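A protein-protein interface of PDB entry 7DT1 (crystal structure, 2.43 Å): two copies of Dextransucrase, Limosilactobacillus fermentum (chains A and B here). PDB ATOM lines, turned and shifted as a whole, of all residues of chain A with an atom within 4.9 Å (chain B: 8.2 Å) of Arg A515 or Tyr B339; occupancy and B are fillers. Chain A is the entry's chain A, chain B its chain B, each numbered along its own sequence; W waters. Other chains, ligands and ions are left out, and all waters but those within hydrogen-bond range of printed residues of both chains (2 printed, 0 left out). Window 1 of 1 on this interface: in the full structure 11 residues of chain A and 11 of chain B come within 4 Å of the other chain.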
ATOM      1  N   GLU A 510     -20.394  -5.792  -5.400  1.00  0.00           N
ATOM      2  CA  GLU A 510     -19.231  -5.646  -4.530  1.00  0.00           C
ATOM      3  C   GLU A 510     -19.452  -6.261  -3.143  1.00  0.00           C
ATOM      4  O   GLU A 510     -18.501  -6.743  -2.516  1.00  0.00           O
ATOM      5  CB  GLU A 510     -18.868  -4.170  -4.402  1.00  0.00           C
ATOM      6  CG  GLU A 510     -18.382  -3.565  -5.684  1.00  0.00           C
ATOM      7  CD  GLU A 510     -17.377  -2.476  -5.443  1.00  0.00           C
ATOM      8  OE1 GLU A 510     -17.471  -1.847  -4.361  1.00  0.00           O
ATOM      9  OE2 GLU A 510     -16.493  -2.268  -6.320  1.00  0.00           O
ATOM     10  N   ASN A 511     -20.678  -6.244  -2.641  1.00  0.00           N
ATOM     11  CA  ASN A 511     -20.915  -6.769  -1.305  1.00  0.00           C
ATOM     12  C   ASN A 511     -21.015  -8.285  -1.298  1.00  0.00           C
ATOM     13  O   ASN A 511     -20.698  -8.914  -0.289  1.00  0.00           O
ATOM     14  CB  ASN A 511     -22.190  -6.162  -0.727  1.00  0.00           C
ATOM     15  CG  ASN A 511     -22.099  -4.657  -0.563  1.00  0.00           C
ATOM     16  OD1 ASN A 511     -21.020  -4.074  -0.613  1.00  0.00           O
ATOM     17  ND2 ASN A 511     -23.239  -4.023  -0.349  1.00  0.00           N
ATOM     18  N   LEU A 513     -19.757 -10.483  -3.986  1.00  0.00           N
ATOM     19  CA  LEU A 513     -18.605 -11.141  -4.595  1.00  0.00           C
ATOM     20  C   LEU A 513     -17.298 -10.422  -4.358  1.00  0.00           C
ATOM     21  O   LEU A 513     -16.248 -11.072  -4.314  1.00  0.00           O
ATOM     22  CB  LEU A 513     -18.808 -11.288  -6.104  1.00  0.00           C
ATOM     23  CG  LEU A 513     -20.126 -11.958  -6.480  1.00  0.00           C
ATOM     24  CD1 LEU A 513     -20.416 -11.813  -7.970  1.00  0.00           C
ATOM     25  CD2 LEU A 513     -20.089 -13.419  -6.066  1.00  0.00           C
ATOM     26  N   GLY A 514     -17.338  -9.103  -4.161  1.00  0.00           N
ATOM     27  CA  GLY A 514     -16.110  -8.331  -4.148  1.00  0.00           C
ATOM     28  C   GLY A 514     -15.366  -8.305  -2.833  1.00  0.00           C
ATOM     29  O   GLY A 514     -14.149  -8.102  -2.844  1.00  0.00           O
ATOM     30  N   ARG A 515     -16.064  -8.497  -1.708  1.00  0.00           N
ATOM     31  CA  ARG A 515     -15.469  -8.381  -0.375  1.00  0.00           C
ATOM     32  C   ARG A 515     -14.472  -9.508  -0.081  1.00  0.00           C
ATOM     33  O   ARG A 515     -14.519 -10.596  -0.660  1.00  0.00           O
ATOM     34  CB  ARG A 515     -16.552  -8.407   0.707  1.00  0.00           C
ATOM     35  CG  ARG A 515     -17.202  -7.098   1.034  1.00  0.00           C
ATOM     36  CD  ARG A 515     -18.381  -7.361   1.936  1.00  0.00           C
ATOM     37  NE  ARG A 515     -19.338  -6.255   1.931  1.00  0.00           N
ATOM     38  CZ  ARG A 515     -20.566  -6.324   2.435  1.00  0.00           C
ATOM     39  NH1 ARG A 515     -21.009  -7.449   2.978  1.00  0.00           N
ATOM     40  NH2 ARG A 515     -21.356  -5.266   2.388  1.00  0.00           N
ATOM     41  N   ALA A 516     -13.583  -9.246   0.872  1.00  0.00           N
ATOM     42  CA  ALA A 516     -12.679 -10.298   1.321  1.00  0.00           C
ATOM     43  C   ALA A 516     -13.396 -11.291   2.221  1.00  0.00           C
ATOM     44  O   ALA A 516     -13.154 -12.496   2.140  1.00  0.00           O
ATOM     45  CB  ALA A 516     -11.494  -9.693   2.059  1.00  0.00           C
ATOM     46  N   SER A 517     -14.277 -10.806   3.084  1.00  0.00           N
ATOM     47  CA  SER A 517     -14.960 -11.655   4.043  1.00  0.00           C
ATOM     48  C   SER A 517     -16.301 -11.019   4.370  1.00  0.00           C
ATOM     49  O   SER A 517     -16.579  -9.883   3.984  1.00  0.00           O
ATOM     50  CB  SER A 517     -14.125 -11.845   5.311  1.00  0.00           C
ATOM     51  OG  SER A 517     -13.946 -10.602   5.982  1.00  0.00           O
ATOM     52  N   ASP A 518     -17.131 -11.770   5.095  1.00  0.00           N
ATOM     53  CA  ASP A 518     -18.476 -11.323   5.451  1.00  0.00           C
ATOM     54  C   ASP A 518     -19.251 -10.905   4.204  1.00  0.00           C
ATOM     55  O   ASP A 518     -19.952  -9.893   4.194  1.00  0.00           O
ATOM     56  CB  ASP A 518     -18.431 -10.176   6.475  1.00  0.00           C
ATOM     57  CG  ASP A 518     -17.502 -10.464   7.659  1.00  0.00           C
ATOM     58  OD1 ASP A 518     -17.706 -11.485   8.360  1.00  0.00           O
ATOM     59  OD2 ASP A 518     -16.559  -9.667   7.882  1.00  0.00           O
ATOM     60  N   ARG A 519     -19.087 -11.671   3.125  1.00  0.00           N
ATOM     61  CA  ARG A 519     -19.852 -11.433   1.908  1.00  0.00           C
ATOM     62  C   ARG A 519     -21.340 -11.617   2.169  1.00  0.00           C
ATOM     63  O   ARG A 519     -21.757 -12.421   3.012  1.00  0.00           O
ATOM     64  CB  ARG A 519     -19.398 -12.370   0.782  1.00  0.00           C
ATOM     65  CG  ARG A 519     -18.004 -12.087   0.334  1.00  0.00           C
ATOM     66  CD  ARG A 519     -17.454 -13.155  -0.569  1.00  0.00           C
ATOM     67  NE  ARG A 519     -16.084 -12.808  -0.914  1.00  0.00           N
ATOM     68  CZ  ARG A 519     -15.180 -13.671  -1.348  1.00  0.00           C
ATOM     69  NH1 ARG A 519     -15.497 -14.944  -1.493  1.00  0.00           N
ATOM     70  NH2 ARG A 519     -13.958 -13.248  -1.625  1.00  0.00           N
ATOM     71  N   ASP A 520     -22.140 -10.861   1.427  1.00  0.00           N
ATOM     72  CA  ASP A 520     -23.573 -10.874   1.617  1.00  0.00           C
ATOM     73  C   ASP A 520     -24.188 -12.089   0.937  1.00  0.00           C
ATOM     74  O   ASP A 520     -23.514 -12.843   0.223  1.00  0.00           O
ATOM     75  CB  ASP A 520     -24.175  -9.574   1.097  1.00  0.00           C
ATOM     76  CG  ASP A 520     -24.009  -8.464   2.070  1.00  0.00           C
ATOM     77  OD1 ASP A 520     -23.524  -8.751   3.189  1.00  0.00           O
ATOM     78  OD2 ASP A 520     -24.359  -7.323   1.737  1.00  0.00           O
ATOM     79  N   TYR A 604     -12.527  -8.887  -5.123  1.00  0.00           N
ATOM     80  CA  TYR A 604     -12.579 -10.315  -5.367  1.00  0.00           C
ATOM     81  C   TYR A 604     -13.568 -10.614  -6.488  1.00  0.00           C
ATOM     82  O   TYR A 604     -14.523  -9.865  -6.722  1.00  0.00           O
ATOM     83  CB  TYR A 604     -12.984 -11.071  -4.097  1.00  0.00           C
ATOM     84  CG  TYR A 604     -11.907 -11.056  -3.043  1.00  0.00           C
ATOM     85  CD1 TYR A 604     -11.595  -9.881  -2.382  1.00  0.00           C
ATOM     86  CD2 TYR A 604     -11.168 -12.202  -2.732  1.00  0.00           C
ATOM     87  CE1 TYR A 604     -10.606  -9.831  -1.445  1.00  0.00           C
ATOM     88  CE2 TYR A 604     -10.151 -12.158  -1.771  1.00  0.00           C
ATOM     89  CZ  TYR A 604      -9.890 -10.958  -1.136  1.00  0.00           C
ATOM     90  OH  TYR A 604      -8.920 -10.833  -0.188  1.00  0.00           O
ATOM     91  N   SER B 334     -30.648  -7.161  12.892  1.00  0.00           N
ATOM     92  CA  SER B 334     -30.050  -6.102  13.699  1.00  0.00           C
ATOM     93  C   SER B 334     -28.897  -5.465  12.943  1.00  0.00           C
ATOM     94  O   SER B 334     -28.062  -6.165  12.357  1.00  0.00           O
ATOM     95  CB  SER B 334     -29.553  -6.658  15.032  1.00  0.00           C
ATOM     96  OG  SER B 334     -28.790  -5.694  15.743  1.00  0.00           O
ATOM     97  N   VAL B 335     -28.859  -4.131  12.926  1.00  0.00           N
ATOM     98  CA  VAL B 335     -27.787  -3.471  12.188  1.00  0.00           C
ATOM     99  C   VAL B 335     -26.451  -3.599  12.896  1.00  0.00           C
ATOM    100  O   VAL B 335     -25.410  -3.347  12.274  1.00  0.00           O
ATOM    101  CB  VAL B 335     -28.099  -1.986  11.905  1.00  0.00           C
ATOM    102  CG1 VAL B 335     -29.420  -1.837  11.108  1.00  0.00           C
ATOM    103  CG2 VAL B 335     -28.107  -1.169  13.191  1.00  0.00           C
ATOM    104  N   VAL B 336     -26.449  -4.021  14.165  1.00  0.00           N
ATOM    105  CA  VAL B 336     -25.188  -4.301  14.848  1.00  0.00           C
ATOM    106  C   VAL B 336     -24.376  -5.316  14.062  1.00  0.00           C
ATOM    107  O   VAL B 336     -23.138  -5.240  14.004  1.00  0.00           O
ATOM    108  CB  VAL B 336     -25.444  -4.780  16.289  1.00  0.00           C
ATOM    109  CG1 VAL B 336     -24.130  -5.135  16.963  1.00  0.00           C
ATOM    110  CG2 VAL B 336     -26.164  -3.699  17.067  1.00  0.00           C
ATOM    111  N   ASN B 337     -25.054  -6.284  13.449  1.00  0.00           N
ATOM    112  CA  ASN B 337     -24.376  -7.334  12.701  1.00  0.00           C
ATOM    113  C   ASN B 337     -24.111  -6.969  11.244  1.00  0.00           C
ATOM    114  O   ASN B 337     -23.589  -7.807  10.516  1.00  0.00           O
ATOM    115  CB  ASN B 337     -25.179  -8.641  12.745  1.00  0.00           C
ATOM    116  CG  ASN B 337     -25.661  -9.002  14.158  1.00  0.00           C
ATOM    117  OD1 ASN B 337     -26.769  -9.530  14.330  1.00  0.00           O
ATOM    118  ND2 ASN B 337     -24.846  -8.706  15.164  1.00  0.00           N
ATOM    119  N   SER B 338     -24.445  -5.756  10.802  1.00  0.00           N
ATOM    120  CA  SER B 338     -24.280  -5.398   9.403  1.00  0.00           C
ATOM    121  C   SER B 338     -22.807  -5.142   9.093  1.00  0.00           C
ATOM    122  O   SER B 338     -21.982  -4.967   9.986  1.00  0.00           O
ATOM    123  CB  SER B 338     -25.122  -4.172   9.044  1.00  0.00           C
ATOM    124  OG  SER B 338     -24.690  -3.005   9.731  1.00  0.00           O
ATOM    125  N   TYR B 339     -22.484  -5.114   7.803  1.00  0.00           N
ATOM    126  CA  TYR B 339     -21.097  -4.978   7.384  1.00  0.00           C
ATOM    127  C   TYR B 339     -20.608  -3.562   7.667  1.00  0.00           C
ATOM    128  O   TYR B 339     -21.207  -2.586   7.197  1.00  0.00           O
ATOM    129  CB  TYR B 339     -20.957  -5.322   5.897  1.00  0.00           C
ATOM    130  CG  TYR B 339     -19.525  -5.379   5.435  1.00  0.00           C
ATOM    131  CD1 TYR B 339     -18.759  -6.528   5.617  1.00  0.00           C
ATOM    132  CD2 TYR B 339     -18.920  -4.275   4.846  1.00  0.00           C
ATOM    133  CE1 TYR B 339     -17.418  -6.581   5.212  1.00  0.00           C
ATOM    134  CE2 TYR B 339     -17.585  -4.316   4.438  1.00  0.00           C
ATOM    135  CZ  TYR B 339     -16.840  -5.470   4.617  1.00  0.00           C
ATOM    136  OH  TYR B 339     -15.519  -5.503   4.205  1.00  0.00           O
ATOM    137  N   GLY B 340     -19.530  -3.447   8.446  1.00  0.00           N
ATOM    138  CA  GLY B 340     -18.989  -2.147   8.787  1.00  0.00           C
ATOM    139  C   GLY B 340     -19.667  -1.410   9.932  1.00  0.00           C
ATOM    140  O   GLY B 340     -19.399  -0.218  10.120  1.00  0.00           O
ATOM    141  N   TYR B 341     -20.528  -2.068  10.707  1.00  0.00           N
ATOM    142  CA  TYR B 341     -21.209  -1.387  11.798  1.00  0.00           C
ATOM    143  C   TYR B 341     -20.225  -0.867  12.841  1.00  0.00           C
ATOM    144  O   TYR B 341     -19.326  -1.587  13.282  1.00  0.00           O
ATOM    145  CB  TYR B 341     -22.206  -2.329  12.463  1.00  0.00           C
ATOM    146  CG  TYR B 341     -22.923  -1.668  13.606  1.00  0.00           C
ATOM    147  CD1 TYR B 341     -24.002  -0.814  13.373  1.00  0.00           C
ATOM    148  CD2 TYR B 341     -22.518  -1.874  14.929  1.00  0.00           C
ATOM    149  CE1 TYR B 341     -24.667  -0.196  14.418  1.00  0.00           C
ATOM    150  CE2 TYR B 341     -23.180  -1.255  15.989  1.00  0.00           C
ATOM    151  CZ  TYR B 341     -24.251  -0.418  15.717  1.00  0.00           C
ATOM    152  OH  TYR B 341     -24.916   0.194  16.742  1.00  0.00           O
ATOM    153  N   LYS B 342     -20.410   0.377  13.248  1.00  0.00           N
ATOM    154  CA  LYS B 342     -19.714   0.997  14.370  1.00  0.00           C
ATOM    155  C   LYS B 342     -20.687   1.249  15.522  1.00  0.00           C
ATOM    156  O   LYS B 342     -21.816   1.699  15.287  1.00  0.00           O
ATOM    157  CB  LYS B 342     -19.065   2.329  13.961  1.00  0.00           C
ATOM    158  CG  LYS B 342     -18.067   2.271  12.794  1.00  0.00           C
ATOM    159  CD  LYS B 342     -16.625   2.079  13.262  1.00  0.00           C
ATOM    160  CE  LYS B 342     -16.286   0.600  13.471  1.00  0.00           C
ATOM    161  NZ  LYS B 342     -14.807   0.330  13.616  1.00  0.00           N
ATOM    162  N   VAL B 930     -30.890  -4.396   5.387  1.00  0.00           N
ATOM    163  CA  VAL B 930     -29.660  -4.641   6.156  1.00  0.00           C
ATOM    164  C   VAL B 930     -28.880  -5.769   5.492  1.00  0.00           C
ATOM    165  O   VAL B 930     -29.371  -6.905   5.426  1.00  0.00           O
ATOM    166  CB  VAL B 930     -29.946  -5.011   7.625  1.00  0.00           C
ATOM    167  CG1 VAL B 930     -28.644  -5.112   8.421  1.00  0.00           C
ATOM    168  CG2 VAL B 930     -30.865  -4.015   8.261  1.00  0.00           C
ATOM    169  N   ASP B 931     -27.646  -5.473   5.052  1.00  0.00           N
ATOM    170  CA  ASP B 931     -26.830  -6.429   4.298  1.00  0.00           C
ATOM    171  C   ASP B 931     -27.638  -7.025   3.145  1.00  0.00           C
ATOM    172  O   ASP B 931     -27.560  -8.220   2.843  1.00  0.00           O
ATOM    173  CB  ASP B 931     -26.276  -7.536   5.203  1.00  0.00           C
ATOM    174  CG  ASP B 931     -25.201  -7.051   6.169  1.00  0.00           C
ATOM    175  OD1 ASP B 931     -24.551  -6.005   5.940  1.00  0.00           O
ATOM    176  OD2 ASP B 931     -24.973  -7.761   7.161  1.00  0.00           O
ATOM    177  N   GLY B 932     -28.459  -6.179   2.516  1.00  0.00           N
ATOM    178  CA  GLY B 932     -29.282  -6.582   1.401  1.00  0.00           C
ATOM    179  C   GLY B 932     -30.580  -7.265   1.764  1.00  0.00           C
ATOM    180  O   GLY B 932     -31.308  -7.686   0.852  1.00  0.00           O
HETATM  181  O   HOH W   1     -23.884  -5.035   3.355  1.00  0.00           O
HETATM  182  O   HOH W   2     -13.721  -7.658   3.909  1.00  0.00           O
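Arg A515 touches just one residue of chain B: Tyr B339. Of chain A, only Arg A515, Ser A517 and Asp A518 come within 4 Å of Tyr B339. No residue of chain B comes within 4 Å of Gly A514. Ala A516 touches none of the printed residues of chain B. Printed residues of chain A within 4 Å of Asp B931: Asp A520 (3.5 Å). Printed residues of chain B within 4 Å of Asp A518: Tyr B339 (3.8 Å). The nearest printed residue of chain A that does not touch Tyr B339 is Asp A520 (5.1 Å). The nearest printed residue of chain B that does not touch Asp A520 is Gly B932 (4.3 Å).
Water W1 lies within hydrogen-bond range of the guanidinium group of Arg A515, the side-chain carboxylate of Asp B931 and the side-chain carboxylate of Asp A520. Water W2 lies within hydrogen-bond range of the side-chain hydroxyl (OH) of Tyr B339 (2.8 Å), the backbone NH (N) of Ser A517 (3.3 Å) and the backbone NH (N) of Ala A516 (3.4 Å).
Among the printed residues, merely in contact across the chains: Arg A515 with Tyr B339 (3.3 Å), Ser A517 with Tyr B339 (3.6 Å), Asp A518 with Tyr B339 (3.8 Å) and Asp A520 with Asp B931 (3.5 Å).
Of the 12 printed residues of chain B, 2 touch a printed residue of chain A. Printed residues of chain B that touch a printed residue of chain A: Tyr B339 and Asp B931. Hydrophobic or aromatic side chains of chain B that line the printed part of chain A: Tyr B339.
The guanidinium group of Arg A515 sits at hydrogen-bond distance from the backbone carbonyl oxygen of Asp A518 (2.9 Å). The side-chain hydroxyl (OG) of Ser A517 is in hydrogen-bond range of the side-chain carboxylate (OD2) of Asp A518, 3.4 Å away. NE of Arg A519 lies within hydrogen-bond range of O of Arg A515 (2.7 Å). The backbone carbonyl oxygen (O) of Glu A510 is in hydrogen-bond range of the backbone NH (N) of Arg A515 (3.1 Å). NH1 of Arg A515 lies within salt-bridge range of OD1 of Asp A520, 2.8 Å away. The side-chain carboxylate of Asp B931 lies within hydrogen-bond range of the backbone NH of Tyr B339 (2.9 Å).
No position is printed for both chains. Of the 4 pairs that touch across the chains among the printed residues, none has its exchanged pair printed and touching as well.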
